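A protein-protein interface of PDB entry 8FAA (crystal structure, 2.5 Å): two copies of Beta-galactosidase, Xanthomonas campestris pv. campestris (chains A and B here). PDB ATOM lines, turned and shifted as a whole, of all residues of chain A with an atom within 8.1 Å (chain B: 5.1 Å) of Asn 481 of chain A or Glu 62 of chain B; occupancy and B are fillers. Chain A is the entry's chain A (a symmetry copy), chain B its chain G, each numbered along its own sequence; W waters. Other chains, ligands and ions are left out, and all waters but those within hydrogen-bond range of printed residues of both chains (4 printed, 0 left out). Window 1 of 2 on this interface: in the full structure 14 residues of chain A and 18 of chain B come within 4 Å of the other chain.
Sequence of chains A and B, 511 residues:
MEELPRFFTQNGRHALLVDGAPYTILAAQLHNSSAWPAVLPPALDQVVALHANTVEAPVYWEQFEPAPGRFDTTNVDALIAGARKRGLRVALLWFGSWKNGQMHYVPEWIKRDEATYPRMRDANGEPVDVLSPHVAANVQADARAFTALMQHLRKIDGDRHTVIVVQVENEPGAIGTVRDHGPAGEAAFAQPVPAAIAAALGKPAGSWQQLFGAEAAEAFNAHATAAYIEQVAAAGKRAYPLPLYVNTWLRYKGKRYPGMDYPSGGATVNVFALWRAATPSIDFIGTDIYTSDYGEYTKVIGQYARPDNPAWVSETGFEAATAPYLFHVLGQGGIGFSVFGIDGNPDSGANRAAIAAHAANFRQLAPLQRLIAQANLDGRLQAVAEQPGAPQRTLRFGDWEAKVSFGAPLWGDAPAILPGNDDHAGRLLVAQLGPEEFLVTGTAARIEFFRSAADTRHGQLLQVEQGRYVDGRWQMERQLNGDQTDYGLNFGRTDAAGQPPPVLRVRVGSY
The backbone NH (N) of Asp 483 of chain A lies within hydrogen-bond range of the side-chain amide oxygen (OD1) of Asn 32 of chain B, at 2.9 Å.
The side-chain hydroxyl (OG) of Ser 33 of chain B lies close to the backbone carbonyl oxygen (O) of Gln 479 of chain A (3.5 Å).
The backbone carbonyl oxygen (O) of Asn 481 of chain A lies within hydrogen-bond range of the side-chain hydroxyl (OG) of Ser 33 of chain B, at 3.2 Å.
The side-chain amide oxygen (OE1) of Gln 484 of chain A lies within hydrogen-bond range of the side-chain hydroxyl (OG) of Ser 33 of chain B, at 2.5 Å.
ND2 of Asn 481 of chain A lies within hydrogen-bond range of OE2 of Glu 62 of chain B (3.3 Å).
The backbone carbonyl oxygen (O) of His 104 of chain B lies within hydrogen-bond range of the side-chain amide nitrogen (ND2) of Asn 481 of chain A (2.7 Å).
OH of Tyr 105 of chain B sits close to O of Asn 481 of chain A (3.2 Å).
OH of Tyr 105 of chain B sits at hydrogen-bond distance from N of Gly 482 of chain A, 3.1 Å away.
The side-chain hydroxyl of Tyr 60 of chain B lies within hydrogen-bond range of the backbone carbonyl oxygen of Asn 32 of chain B (2.6 Å).
The backbone carbonyl oxygen (O) of Tyr 105 of chain B is in hydrogen-bond range of the backbone NH (N) of Glu 62 of chain B.
The side-chain carboxylate of Glu 62 of chain B lies within salt-bridge range of the side-chain amino group of Lys 111 of chain B (3.5 Å).
The backbone carbonyl oxygen (O) of His 104 of chain B lies within hydrogen-bond range of the side-chain amino group (NZ) of Lys 111 of chain B, at 3.3 Å.
OE1 of Gln 479 of chain A lies within hydrogen-bond range of NE2 of Gln 463 of chain A (2.9 Å).
O of Asn 481 of chain A sits close to OE1 of Gln 484 of chain A (3.3 Å).
Arg 478 of chain A touches Ser 33 of chain B.
Ser 33 of chain B touches Leu 480 of chain A (OG to CA, 3.5 Å).
Gly 482 of chain A touches Asn 32 of chain B (C to OD1, 3.9 Å).
Asn 32 of chain B touches Gln 484 of chain A.
Of chain B, only Ser 33, Glu 62, His 104 and Tyr 105 come within 4 Å of Asn 481 of chain A.
Glu 62 of chain B touches just one residue of chain A: Asn 481.
Of the printed residues of chain B, Gly 482 of chain A touches Asn 32 (3.9 Å) and Tyr 105 (3.1 Å).
Of the printed residues of chain A, Asn 32 of chain B touches Gly 482 (3.9 Å), Asp 483 (2.9 Å) and Gln 484 (3.4 Å).
Of the printed residues of chain B, Asp 483 of chain A touches Asn 32.
Lys 111 of chain B touches none of the printed residues of chain A.
The nearest printed residue of chain B that does not touch Asp 483 of chain A is Tyr 105 of chain B (4.8 Å).
Of the 14 printed residues of chain B, 5 touch a printed residue of chain A.
Among the printed residues, no Asp or Glu carboxylate lies within 4 Å of a Lys or Arg side-chain nitrogen of the other chain.
No position is printed for both chains.
Of the 12 pairs that touch across the chains among the printed residues, none has its exchanged pair printed and touching as well.
Water W3 lies within hydrogen-bond range of OH of Tyr 105 of chain B (2.5 Å), OG of Ser 33 of chain B (2.9 Å) and O of Asn 481 of chain A (3.1 Å).
Water W2 lies within hydrogen-bond range of O of Gln 479 of chain A (2.6 Å) and OH of Tyr 60 of chain B (3.5 Å).
Water W4 lies within hydrogen-bond range of OD1 of Asp 486 of chain A (2.6 Å), ND1 of His 104 of chain B (2.8 Å) and O of Gly 482 of chain A (3.2 Å).
Water W1 lies within hydrogen-bond range of the backbone NH (N) of Asn 32 of chain B (2.8 Å), the side-chain carboxylate (OD2) of Asp 483 of chain A (3.0 Å) and the side-chain amide nitrogen (NE2) of Gln 484 of chain A (3.1 Å).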
ATOM      1  N   LEU A 461      -3.561 -29.204  12.373  1.00  0.00           N
ATOM      2  CA  LEU A 461      -3.628 -28.117  11.408  1.00  0.00           C
ATOM      3  C   LEU A 461      -5.004 -27.463  11.469  1.00  0.00           C
ATOM      4  O   LEU A 461      -6.021 -28.138  11.284  1.00  0.00           O
ATOM      5  CB  LEU A 461      -3.351 -28.661  10.007  1.00  0.00           C
ATOM      6  CG  LEU A 461      -2.332 -27.925   9.132  1.00  0.00           C
ATOM      7  CD1 LEU A 461      -0.971 -27.961   9.787  1.00  0.00           C
ATOM      8  CD2 LEU A 461      -2.244 -28.552   7.777  1.00  0.00           C
ATOM      9  N   LEU A 462      -5.043 -26.155  11.722  1.00  0.00           N
ATOM     10  CA  LEU A 462      -6.294 -25.406  11.796  1.00  0.00           C
ATOM     11  C   LEU A 462      -6.654 -24.691  10.495  1.00  0.00           C
ATOM     12  O   LEU A 462      -7.789 -24.818  10.029  1.00  0.00           O
ATOM     13  CB  LEU A 462      -6.241 -24.395  12.950  1.00  0.00           C
ATOM     14  CG  LEU A 462      -6.417 -24.968  14.360  1.00  0.00           C
ATOM     15  CD1 LEU A 462      -6.428 -23.856  15.396  1.00  0.00           C
ATOM     16  CD2 LEU A 462      -7.681 -25.822  14.465  1.00  0.00           C
ATOM     17  N   GLN A 463      -5.719 -23.949   9.895  1.00  0.00           N
ATOM     18  CA  GLN A 463      -6.021 -23.167   8.701  1.00  0.00           C
ATOM     19  C   GLN A 463      -4.753 -22.911   7.894  1.00  0.00           C
ATOM     20  O   GLN A 463      -3.738 -22.479   8.453  1.00  0.00           O
ATOM     21  CB  GLN A 463      -6.666 -21.838   9.082  1.00  0.00           C
ATOM     22  CG  GLN A 463      -7.255 -21.117   7.916  1.00  0.00           C
ATOM     23  CD  GLN A 463      -7.731 -19.748   8.290  1.00  0.00           C
ATOM     24  OE1 GLN A 463      -7.654 -19.357   9.454  1.00  0.00           O
ATOM     25  NE2 GLN A 463      -8.214 -18.996   7.306  1.00  0.00           N
ATOM     26  N   VAL A 464      -4.823 -23.145   6.580  1.00  0.00           N
ATOM     27  CA  VAL A 464      -3.686 -22.991   5.671  1.00  0.00           C
ATOM     28  C   VAL A 464      -4.136 -22.108   4.505  1.00  0.00           C
ATOM     29  O   VAL A 464      -4.836 -22.574   3.596  1.00  0.00           O
ATOM     30  CB  VAL A 464      -3.157 -24.344   5.169  1.00  0.00           C
ATOM     31  CG1 VAL A 464      -2.037 -24.144   4.138  1.00  0.00           C
ATOM     32  CG2 VAL A 464      -2.677 -25.201   6.339  1.00  0.00           C
ATOM     33  N   GLU A 465      -3.719 -20.848   4.508  1.00  0.00           N
ATOM     34  CA  GLU A 465      -4.100 -19.899   3.469  1.00  0.00           C
ATOM     35  C   GLU A 465      -2.996 -19.765   2.424  1.00  0.00           C
ATOM     36  O   GLU A 465      -1.854 -19.416   2.752  1.00  0.00           O
ATOM     37  CB  GLU A 465      -4.420 -18.534   4.071  1.00  0.00           C
ATOM     38  CG  GLU A 465      -5.641 -18.535   4.959  1.00  0.00           C
ATOM     39  CD  GLU A 465      -6.304 -17.173   5.042  1.00  0.00           C
ATOM     40  OE1 GLU A 465      -5.586 -16.149   5.004  1.00  0.00           O
ATOM     41  OE2 GLU A 465      -7.547 -17.136   5.151  1.00  0.00           O
ATOM     42  N   ARG A 478      -6.824 -19.153  -1.868  1.00  0.00           N
ATOM     43  CA  ARG A 478      -7.539 -20.381  -1.550  1.00  0.00           C
ATOM     44  C   ARG A 478      -7.096 -20.857  -0.172  1.00  0.00           C
ATOM     45  O   ARG A 478      -6.143 -20.339   0.411  1.00  0.00           O
ATOM     46  CB  ARG A 478      -7.291 -21.451  -2.617  1.00  0.00           C
ATOM     47  CG  ARG A 478      -5.908 -22.081  -2.562  1.00  0.00           C
ATOM     48  CD  ARG A 478      -5.727 -23.132  -3.636  1.00  0.00           C
ATOM     49  NE  ARG A 478      -5.480 -22.537  -4.945  1.00  0.00           N
ATOM     50  CZ  ARG A 478      -5.730 -23.146  -6.095  1.00  0.00           C
ATOM     51  NH1 ARG A 478      -6.239 -24.366  -6.133  1.00  0.00           N
ATOM     52  NH2 ARG A 478      -5.461 -22.517  -7.233  1.00  0.00           N
ATOM     53  N   GLN A 479      -7.811 -21.842   0.357  1.00  0.00           N
ATOM     54  CA  GLN A 479      -7.385 -22.526   1.572  1.00  0.00           C
ATOM     55  C   GLN A 479      -7.015 -23.956   1.219  1.00  0.00           C
ATOM     56  O   GLN A 479      -7.680 -24.590   0.396  1.00  0.00           O
ATOM     57  CB  GLN A 479      -8.469 -22.499   2.658  1.00  0.00           C
ATOM     58  CG  GLN A 479      -8.819 -21.083   3.124  1.00  0.00           C
ATOM     59  CD  GLN A 479      -9.674 -21.045   4.388  1.00  0.00           C
ATOM     60  OE1 GLN A 479      -9.772 -20.007   5.048  1.00  0.00           O
ATOM     61  NE2 GLN A 479     -10.299 -22.175   4.727  1.00  0.00           N
ATOM     62  N   LEU A 480      -5.927 -24.445   1.808  1.00  0.00           N
ATOM     63  CA  LEU A 480      -5.408 -25.769   1.491  1.00  0.00           C
ATOM     64  C   LEU A 480      -5.885 -26.772   2.535  1.00  0.00           C
ATOM     65  O   LEU A 480      -5.866 -26.486   3.737  1.00  0.00           O
ATOM     66  CB  LEU A 480      -3.880 -25.762   1.431  1.00  0.00           C
ATOM     67  CG  LEU A 480      -3.181 -24.838   0.439  1.00  0.00           C
ATOM     68  CD1 LEU A 480      -1.702 -25.193   0.375  1.00  0.00           C
ATOM     69  CD2 LEU A 480      -3.832 -24.929  -0.936  1.00  0.00           C
ATOM     70  N   ASN A 481      -6.311 -27.944   2.066  1.00  0.00           N
ATOM     71  CA  ASN A 481      -6.800 -29.040   2.902  1.00  0.00           C
ATOM     72  C   ASN A 481      -6.906 -30.272   2.003  1.00  0.00           C
ATOM     73  O   ASN A 481      -6.691 -30.196   0.789  1.00  0.00           O
ATOM     74  CB  ASN A 481      -8.139 -28.684   3.562  1.00  0.00           C
ATOM     75  CG  ASN A 481      -8.444 -29.518   4.803  1.00  0.00           C
ATOM     76  OD1 ASN A 481      -7.887 -30.608   4.999  1.00  0.00           O
ATOM     77  ND2 ASN A 481      -9.348 -29.011   5.645  1.00  0.00           N
ATOM     78  N   GLY A 482      -7.247 -31.413   2.606  1.00  0.00           N
ATOM     79  CA  GLY A 482      -7.397 -32.636   1.834  1.00  0.00           C
ATOM     80  C   GLY A 482      -6.098 -33.029   1.162  1.00  0.00           C
ATOM     81  O   GLY A 482      -5.052 -33.143   1.810  1.00  0.00           O
ATOM     82  N   ASP A 483      -6.160 -33.236  -0.162  1.00  0.00           N
ATOM     83  CA  ASP A 483      -4.981 -33.658  -0.918  1.00  0.00           C
ATOM     84  C   ASP A 483      -3.814 -32.687  -0.733  1.00  0.00           C
ATOM     85  O   ASP A 483      -2.660 -33.112  -0.640  1.00  0.00           O
ATOM     86  CB  ASP A 483      -5.324 -33.792  -2.401  1.00  0.00           C
ATOM     87  CG  ASP A 483      -6.137 -35.033  -2.706  1.00  0.00           C
ATOM     88  OD1 ASP A 483      -6.344 -35.853  -1.790  1.00  0.00           O
ATOM     89  OD2 ASP A 483      -6.576 -35.186  -3.867  1.00  0.00           O
ATOM     90  N   GLN A 484      -4.094 -31.386  -0.667  1.00  0.00           N
ATOM     91  CA  GLN A 484      -3.024 -30.398  -0.569  1.00  0.00           C
ATOM     92  C   GLN A 484      -2.424 -30.315   0.821  1.00  0.00           C
ATOM     93  O   GLN A 484      -1.494 -29.525   1.033  1.00  0.00           O
ATOM     94  CB  GLN A 484      -3.529 -29.020  -0.979  1.00  0.00           C
ATOM     95  CG  GLN A 484      -3.780 -28.884  -2.467  1.00  0.00           C
ATOM     96  CD  GLN A 484      -4.947 -29.732  -2.910  1.00  0.00           C
ATOM     97  OE1 GLN A 484      -6.058 -29.587  -2.396  1.00  0.00           O
ATOM     98  NE2 GLN A 484      -4.703 -30.643  -3.846  1.00  0.00           N
ATOM     99  N   THR A 485      -2.927 -31.112   1.756  1.00  0.00           N
ATOM    100  CA  THR A 485      -2.499 -31.086   3.148  1.00  0.00           C
ATOM    101  C   THR A 485      -2.161 -32.467   3.697  1.00  0.00           C
ATOM    102  O   THR A 485      -1.410 -32.553   4.677  1.00  0.00           O
ATOM    103  CB  THR A 485      -3.593 -30.409   4.004  1.00  0.00           C
ATOM    104  OG1 THR A 485      -3.445 -28.981   3.929  1.00  0.00           O
ATOM    105  CG2 THR A 485      -3.575 -30.827   5.436  1.00  0.00           C
ATOM    106  N   ASP A 486      -2.600 -33.543   3.034  1.00  0.00           N
ATOM    107  CA  ASP A 486      -2.444 -34.905   3.547  1.00  0.00           C
ATOM    108  C   ASP A 486      -0.983 -35.303   3.709  1.00  0.00           C
ATOM    109  O   ASP A 486      -0.636 -36.055   4.629  1.00  0.00           O
ATOM    110  CB  ASP A 486      -3.126 -35.885   2.596  1.00  0.00           C
ATOM    111  CG  ASP A 486      -4.588 -36.073   2.894  1.00  0.00           C
ATOM    112  OD1 ASP A 486      -5.034 -35.709   4.011  1.00  0.00           O
ATOM    113  OD2 ASP A 486      -5.287 -36.595   1.997  1.00  0.00           O
ATOM    114  N   LEU A 489       2.983 -29.821   3.304  1.00  0.00           N
ATOM    115  CA  LEU A 489       2.841 -28.709   2.381  1.00  0.00           C
ATOM    116  C   LEU A 489       3.981 -28.796   1.377  1.00  0.00           C
ATOM    117  O   LEU A 489       5.153 -28.859   1.766  1.00  0.00           O
ATOM    118  CB  LEU A 489       2.848 -27.378   3.131  1.00  0.00           C
ATOM    119  CG  LEU A 489       1.897 -27.312   4.332  1.00  0.00           C
ATOM    120  CD1 LEU A 489       1.890 -25.932   4.981  1.00  0.00           C
ATOM    121  CD2 LEU A 489       0.478 -27.740   3.953  1.00  0.00           C
ATOM    122  N   ASN B  32      -9.054 -30.615  -4.712  1.00  0.00           N
ATOM    123  CA  ASN B  32      -9.743 -30.486  -3.425  1.00  0.00           C
ATOM    124  C   ASN B  32      -9.842 -29.034  -2.968  1.00  0.00           C
ATOM    125  O   ASN B  32     -10.859 -28.627  -2.392  1.00  0.00           O
ATOM    126  CB  ASN B  32      -9.032 -31.306  -2.343  1.00  0.00           C
ATOM    127  CG  ASN B  32      -9.240 -32.802  -2.485  1.00  0.00           C
ATOM    128  OD1 ASN B  32      -8.591 -33.594  -1.791  1.00  0.00           O
ATOM    129  ND2 ASN B  32     -10.127 -33.203  -3.391  1.00  0.00           N
ATOM    130  N   SER B  33      -8.795 -28.242  -3.197  1.00  0.00           N
ATOM    131  CA  SER B  33      -8.715 -26.899  -2.640  1.00  0.00           C
ATOM    132  C   SER B  33      -9.079 -25.823  -3.651  1.00  0.00           C
ATOM    133  O   SER B  33      -8.729 -24.655  -3.449  1.00  0.00           O
ATOM    134  CB  SER B  33      -7.312 -26.635  -2.090  1.00  0.00           C
ATOM    135  OG  SER B  33      -6.941 -27.604  -1.132  1.00  0.00           O
ATOM    136  N   TYR B  60     -17.255 -27.186   1.486  1.00  0.00           N
ATOM    137  CA  TYR B  60     -16.497 -27.473   2.700  1.00  0.00           C
ATOM    138  C   TYR B  60     -17.319 -27.114   3.934  1.00  0.00           C
ATOM    139  O   TYR B  60     -17.711 -25.954   4.108  1.00  0.00           O
ATOM    140  CB  TYR B  60     -15.177 -26.700   2.728  1.00  0.00           C
ATOM    141  CG  TYR B  60     -14.400 -26.625   1.435  1.00  0.00           C
ATOM    142  CD1 TYR B  60     -13.793 -27.753   0.889  1.00  0.00           C
ATOM    143  CD2 TYR B  60     -14.219 -25.412   0.788  1.00  0.00           C
ATOM    144  CE1 TYR B  60     -13.047 -27.677  -0.285  1.00  0.00           C
ATOM    145  CE2 TYR B  60     -13.483 -25.323  -0.389  1.00  0.00           C
ATOM    146  CZ  TYR B  60     -12.897 -26.455  -0.923  1.00  0.00           C
ATOM    147  OH  TYR B  60     -12.167 -26.350  -2.091  1.00  0.00           O
ATOM    148  N   TRP B  61     -17.565 -28.101   4.801  1.00  0.00           N
ATOM    149  CA  TRP B  61     -18.241 -27.824   6.068  1.00  0.00           C
ATOM    150  C   TRP B  61     -17.524 -26.717   6.832  1.00  0.00           C
ATOM    151  O   TRP B  61     -18.156 -25.765   7.307  1.00  0.00           O
ATOM    152  CB  TRP B  61     -18.327 -29.104   6.905  1.00  0.00           C
ATOM    153  CG  TRP B  61     -19.207 -29.011   8.130  1.00  0.00           C
ATOM    154  CD1 TRP B  61     -19.968 -27.940   8.528  1.00  0.00           C
ATOM    155  CD2 TRP B  61     -19.435 -30.042   9.105  1.00  0.00           C
ATOM    156  NE1 TRP B  61     -20.636 -28.238   9.694  1.00  0.00           N
ATOM    157  CE2 TRP B  61     -20.330 -29.522  10.065  1.00  0.00           C
ATOM    158  CE3 TRP B  61     -18.964 -31.350   9.262  1.00  0.00           C
ATOM    159  CZ2 TRP B  61     -20.756 -30.265  11.166  1.00  0.00           C
ATOM    160  CZ3 TRP B  61     -19.395 -32.086  10.357  1.00  0.00           C
ATOM    161  CH2 TRP B  61     -20.278 -31.539  11.292  1.00  0.00           C
ATOM    162  N   GLU B  62     -16.199 -26.840   6.954  1.00  0.00           N
ATOM    163  CA  GLU B  62     -15.283 -25.810   7.438  1.00  0.00           C
ATOM    164  C   GLU B  62     -15.720 -24.379   7.178  1.00  0.00           C
ATOM    165  O   GLU B  62     -15.771 -23.566   8.107  1.00  0.00           O
ATOM    166  CB  GLU B  62     -13.910 -25.963   6.787  1.00  0.00           C
ATOM    167  CG  GLU B  62     -12.889 -26.743   7.540  1.00  0.00           C
ATOM    168  CD  GLU B  62     -11.523 -26.591   6.909  1.00  0.00           C
ATOM    169  OE1 GLU B  62     -11.478 -26.379   5.683  1.00  0.00           O
ATOM    170  OE2 GLU B  62     -10.501 -26.681   7.629  1.00  0.00           O
ATOM    171  N   GLN B  63     -15.955 -24.034   5.904  1.00  0.00           N
ATOM    172  CA  GLN B  63     -16.323 -22.663   5.572  1.00  0.00           C
ATOM    173  C   GLN B  63     -17.829 -22.465   5.515  1.00  0.00           C
ATOM    174  O   GLN B  63     -18.305 -21.341   5.711  1.00  0.00           O
ATOM    175  CB  GLN B  63     -15.671 -22.225   4.244  1.00  0.00           C
ATOM    176  CG  GLN B  63     -16.431 -22.582   2.962  1.00  0.00           C
ATOM    177  CD  GLN B  63     -17.548 -21.601   2.616  1.00  0.00           C
ATOM    178  OE1 GLN B  63     -17.435 -20.391   2.829  1.00  0.00           O
ATOM    179  NE2 GLN B  63     -18.639 -22.132   2.088  1.00  0.00           N
ATOM    180  N   PHE B  64     -18.587 -23.528   5.256  1.00  0.00           N
ATOM    181  CA  PHE B  64     -20.037 -23.395   5.169  1.00  0.00           C
ATOM    182  C   PHE B  64     -20.662 -23.114   6.534  1.00  0.00           C
ATOM    183  O   PHE B  64     -21.627 -22.346   6.626  1.00  0.00           O
ATOM    184  CB  PHE B  64     -20.641 -24.646   4.543  1.00  0.00           C
ATOM    185  CG  PHE B  64     -22.135 -24.617   4.458  1.00  0.00           C
ATOM    186  CD1 PHE B  64     -22.776 -23.641   3.724  1.00  0.00           C
ATOM    187  CD2 PHE B  64     -22.902 -25.581   5.088  1.00  0.00           C
ATOM    188  CE1 PHE B  64     -24.148 -23.614   3.636  1.00  0.00           C
ATOM    189  CE2 PHE B  64     -24.269 -25.557   4.994  1.00  0.00           C
ATOM    190  CZ  PHE B  64     -24.892 -24.569   4.265  1.00  0.00           C
ATOM    191  N   GLU B  65     -20.133 -23.709   7.610  1.00  0.00           N
ATOM    192  CA  GLU B  65     -20.601 -23.419   8.970  1.00  0.00           C
ATOM    193  C   GLU B  65     -19.430 -22.930   9.823  1.00  0.00           C
ATOM    194  O   GLU B  65     -18.904 -23.678  10.657  1.00  0.00           O
ATOM    195  CB  GLU B  65     -21.288 -24.633   9.608  1.00  0.00           C
ATOM    196  CG  GLU B  65     -22.086 -24.275  10.871  1.00  0.00           C
ATOM    197  CD  GLU B  65     -22.876 -25.428  11.490  1.00  0.00           C
ATOM    198  OE1 GLU B  65     -22.650 -26.616  11.157  1.00  0.00           O
ATOM    199  OE2 GLU B  65     -23.729 -25.126  12.347  1.00  0.00           O
ATOM    200  N   PRO B  66     -19.018 -21.663   9.668  1.00  0.00           N
ATOM    201  CA  PRO B  66     -17.853 -21.155  10.422  1.00  0.00           C
ATOM    202  C   PRO B  66     -18.130 -20.885  11.899  1.00  0.00           C
ATOM    203  O   PRO B  66     -17.176 -20.670  12.660  1.00  0.00           O
ATOM    204  CB  PRO B  66     -17.514 -19.849   9.696  1.00  0.00           C
ATOM    205  CG  PRO B  66     -18.820 -19.384   9.173  1.00  0.00           C
ATOM    206  CD  PRO B  66     -19.625 -20.613   8.829  1.00  0.00           C
ATOM    207  N   HIS B 104     -10.712 -33.764   8.464  1.00  0.00           N
ATOM    208  CA  HIS B 104     -10.010 -32.483   8.342  1.00  0.00           C
ATOM    209  C   HIS B 104     -10.877 -31.372   7.763  1.00  0.00           C
ATOM    210  O   HIS B 104     -10.439 -30.220   7.760  1.00  0.00           O
ATOM    211  CB  HIS B 104      -8.746 -32.625   7.489  1.00  0.00           C
ATOM    212  CG  HIS B 104      -7.704 -33.506   8.098  1.00  0.00           C
ATOM    213  ND1 HIS B 104      -6.675 -34.056   7.366  1.00  0.00           N
ATOM    214  CD2 HIS B 104      -7.532 -33.935   9.371  1.00  0.00           C
ATOM    215  CE1 HIS B 104      -5.924 -34.803   8.157  1.00  0.00           C
ATOM    216  NE2 HIS B 104      -6.424 -34.746   9.378  1.00  0.00           N
ATOM    217  N   TYR B 105     -12.077 -31.670   7.275  1.00  0.00           N
ATOM    218  CA  TYR B 105     -12.961 -30.632   6.760  1.00  0.00           C
ATOM    219  C   TYR B 105     -14.045 -30.245   7.759  1.00  0.00           C
ATOM    220  O   TYR B 105     -14.873 -29.369   7.475  1.00  0.00           O
ATOM    221  CB  TYR B 105     -13.570 -31.082   5.431  1.00  0.00           C
ATOM    222  CG  TYR B 105     -12.585 -30.942   4.288  1.00  0.00           C
ATOM    223  CD1 TYR B 105     -12.518 -29.769   3.537  1.00  0.00           C
ATOM    224  CD2 TYR B 105     -11.690 -31.970   3.985  1.00  0.00           C
ATOM    225  CE1 TYR B 105     -11.602 -29.630   2.506  1.00  0.00           C
ATOM    226  CE2 TYR B 105     -10.776 -31.838   2.960  1.00  0.00           C
ATOM    227  CZ  TYR B 105     -10.739 -30.668   2.222  1.00  0.00           C
ATOM    228  OH  TYR B 105      -9.838 -30.534   1.204  1.00  0.00           O
ATOM    229  N   VAL B 106     -14.039 -30.872   8.926  1.00  0.00           N
ATOM    230  CA  VAL B 106     -14.930 -30.519  10.031  1.00  0.00           C
ATOM    231  C   VAL B 106     -14.616 -29.107  10.518  1.00  0.00           C
ATOM    232  O   VAL B 106     -13.431 -28.712  10.542  1.00  0.00           O
ATOM    233  CB  VAL B 106     -14.769 -31.558  11.147  1.00  0.00           C
ATOM    234  CG1 VAL B 106     -14.899 -30.940  12.479  1.00  0.00           C
ATOM    235  CG2 VAL B 106     -15.785 -32.684  10.957  1.00  0.00           C
ATOM    236  N   PRO B 107     -15.607 -28.301  10.915  1.00  0.00           N
ATOM    237  CA  PRO B 107     -15.329 -26.903  11.273  1.00  0.00           C
ATOM    238  C   PRO B 107     -14.397 -26.777  12.472  1.00  0.00           C
ATOM    239  O   PRO B 107     -14.166 -27.727  13.224  1.00  0.00           O
ATOM    240  CB  PRO B 107     -16.715 -26.337  11.594  1.00  0.00           C
ATOM    241  CG  PRO B 107     -17.673 -27.253  10.907  1.00  0.00           C
ATOM    242  CD  PRO B 107     -17.046 -28.607  10.960  1.00  0.00           C
ATOM    243  N   LYS B 111     -13.191 -28.946  15.916  1.00  0.00           N
ATOM    244  CA  LYS B 111     -11.795 -29.344  16.103  1.00  0.00           C
ATOM    245  C   LYS B 111     -11.243 -28.898  17.455  1.00  0.00           C
ATOM    246  O   LYS B 111     -10.377 -29.574  18.018  1.00  0.00           O
ATOM    247  CB  LYS B 111     -10.928 -28.773  14.980  1.00  0.00           C
ATOM    248  CG  LYS B 111     -10.941 -29.588  13.697  1.00  0.00           C
ATOM    249  CD  LYS B 111      -9.662 -29.378  12.900  1.00  0.00           C
ATOM    250  CE  LYS B 111      -9.833 -29.775  11.439  1.00  0.00           C
ATOM    251  NZ  LYS B 111     -10.194 -28.613  10.589  1.00  0.00           N
HETATM  252  O   HOH W   1      -6.991 -32.430  -4.987  1.00  0.00           O
HETATM  253  O   HOH W   2      -9.969 -25.718   0.527  1.00  0.00           O
HETATM  254  O   HOH W   3      -9.112 -28.224   0.619  1.00  0.00           O
HETATM  255  O   HOH W   4      -5.405 -33.265   4.964  1.00  0.00           O
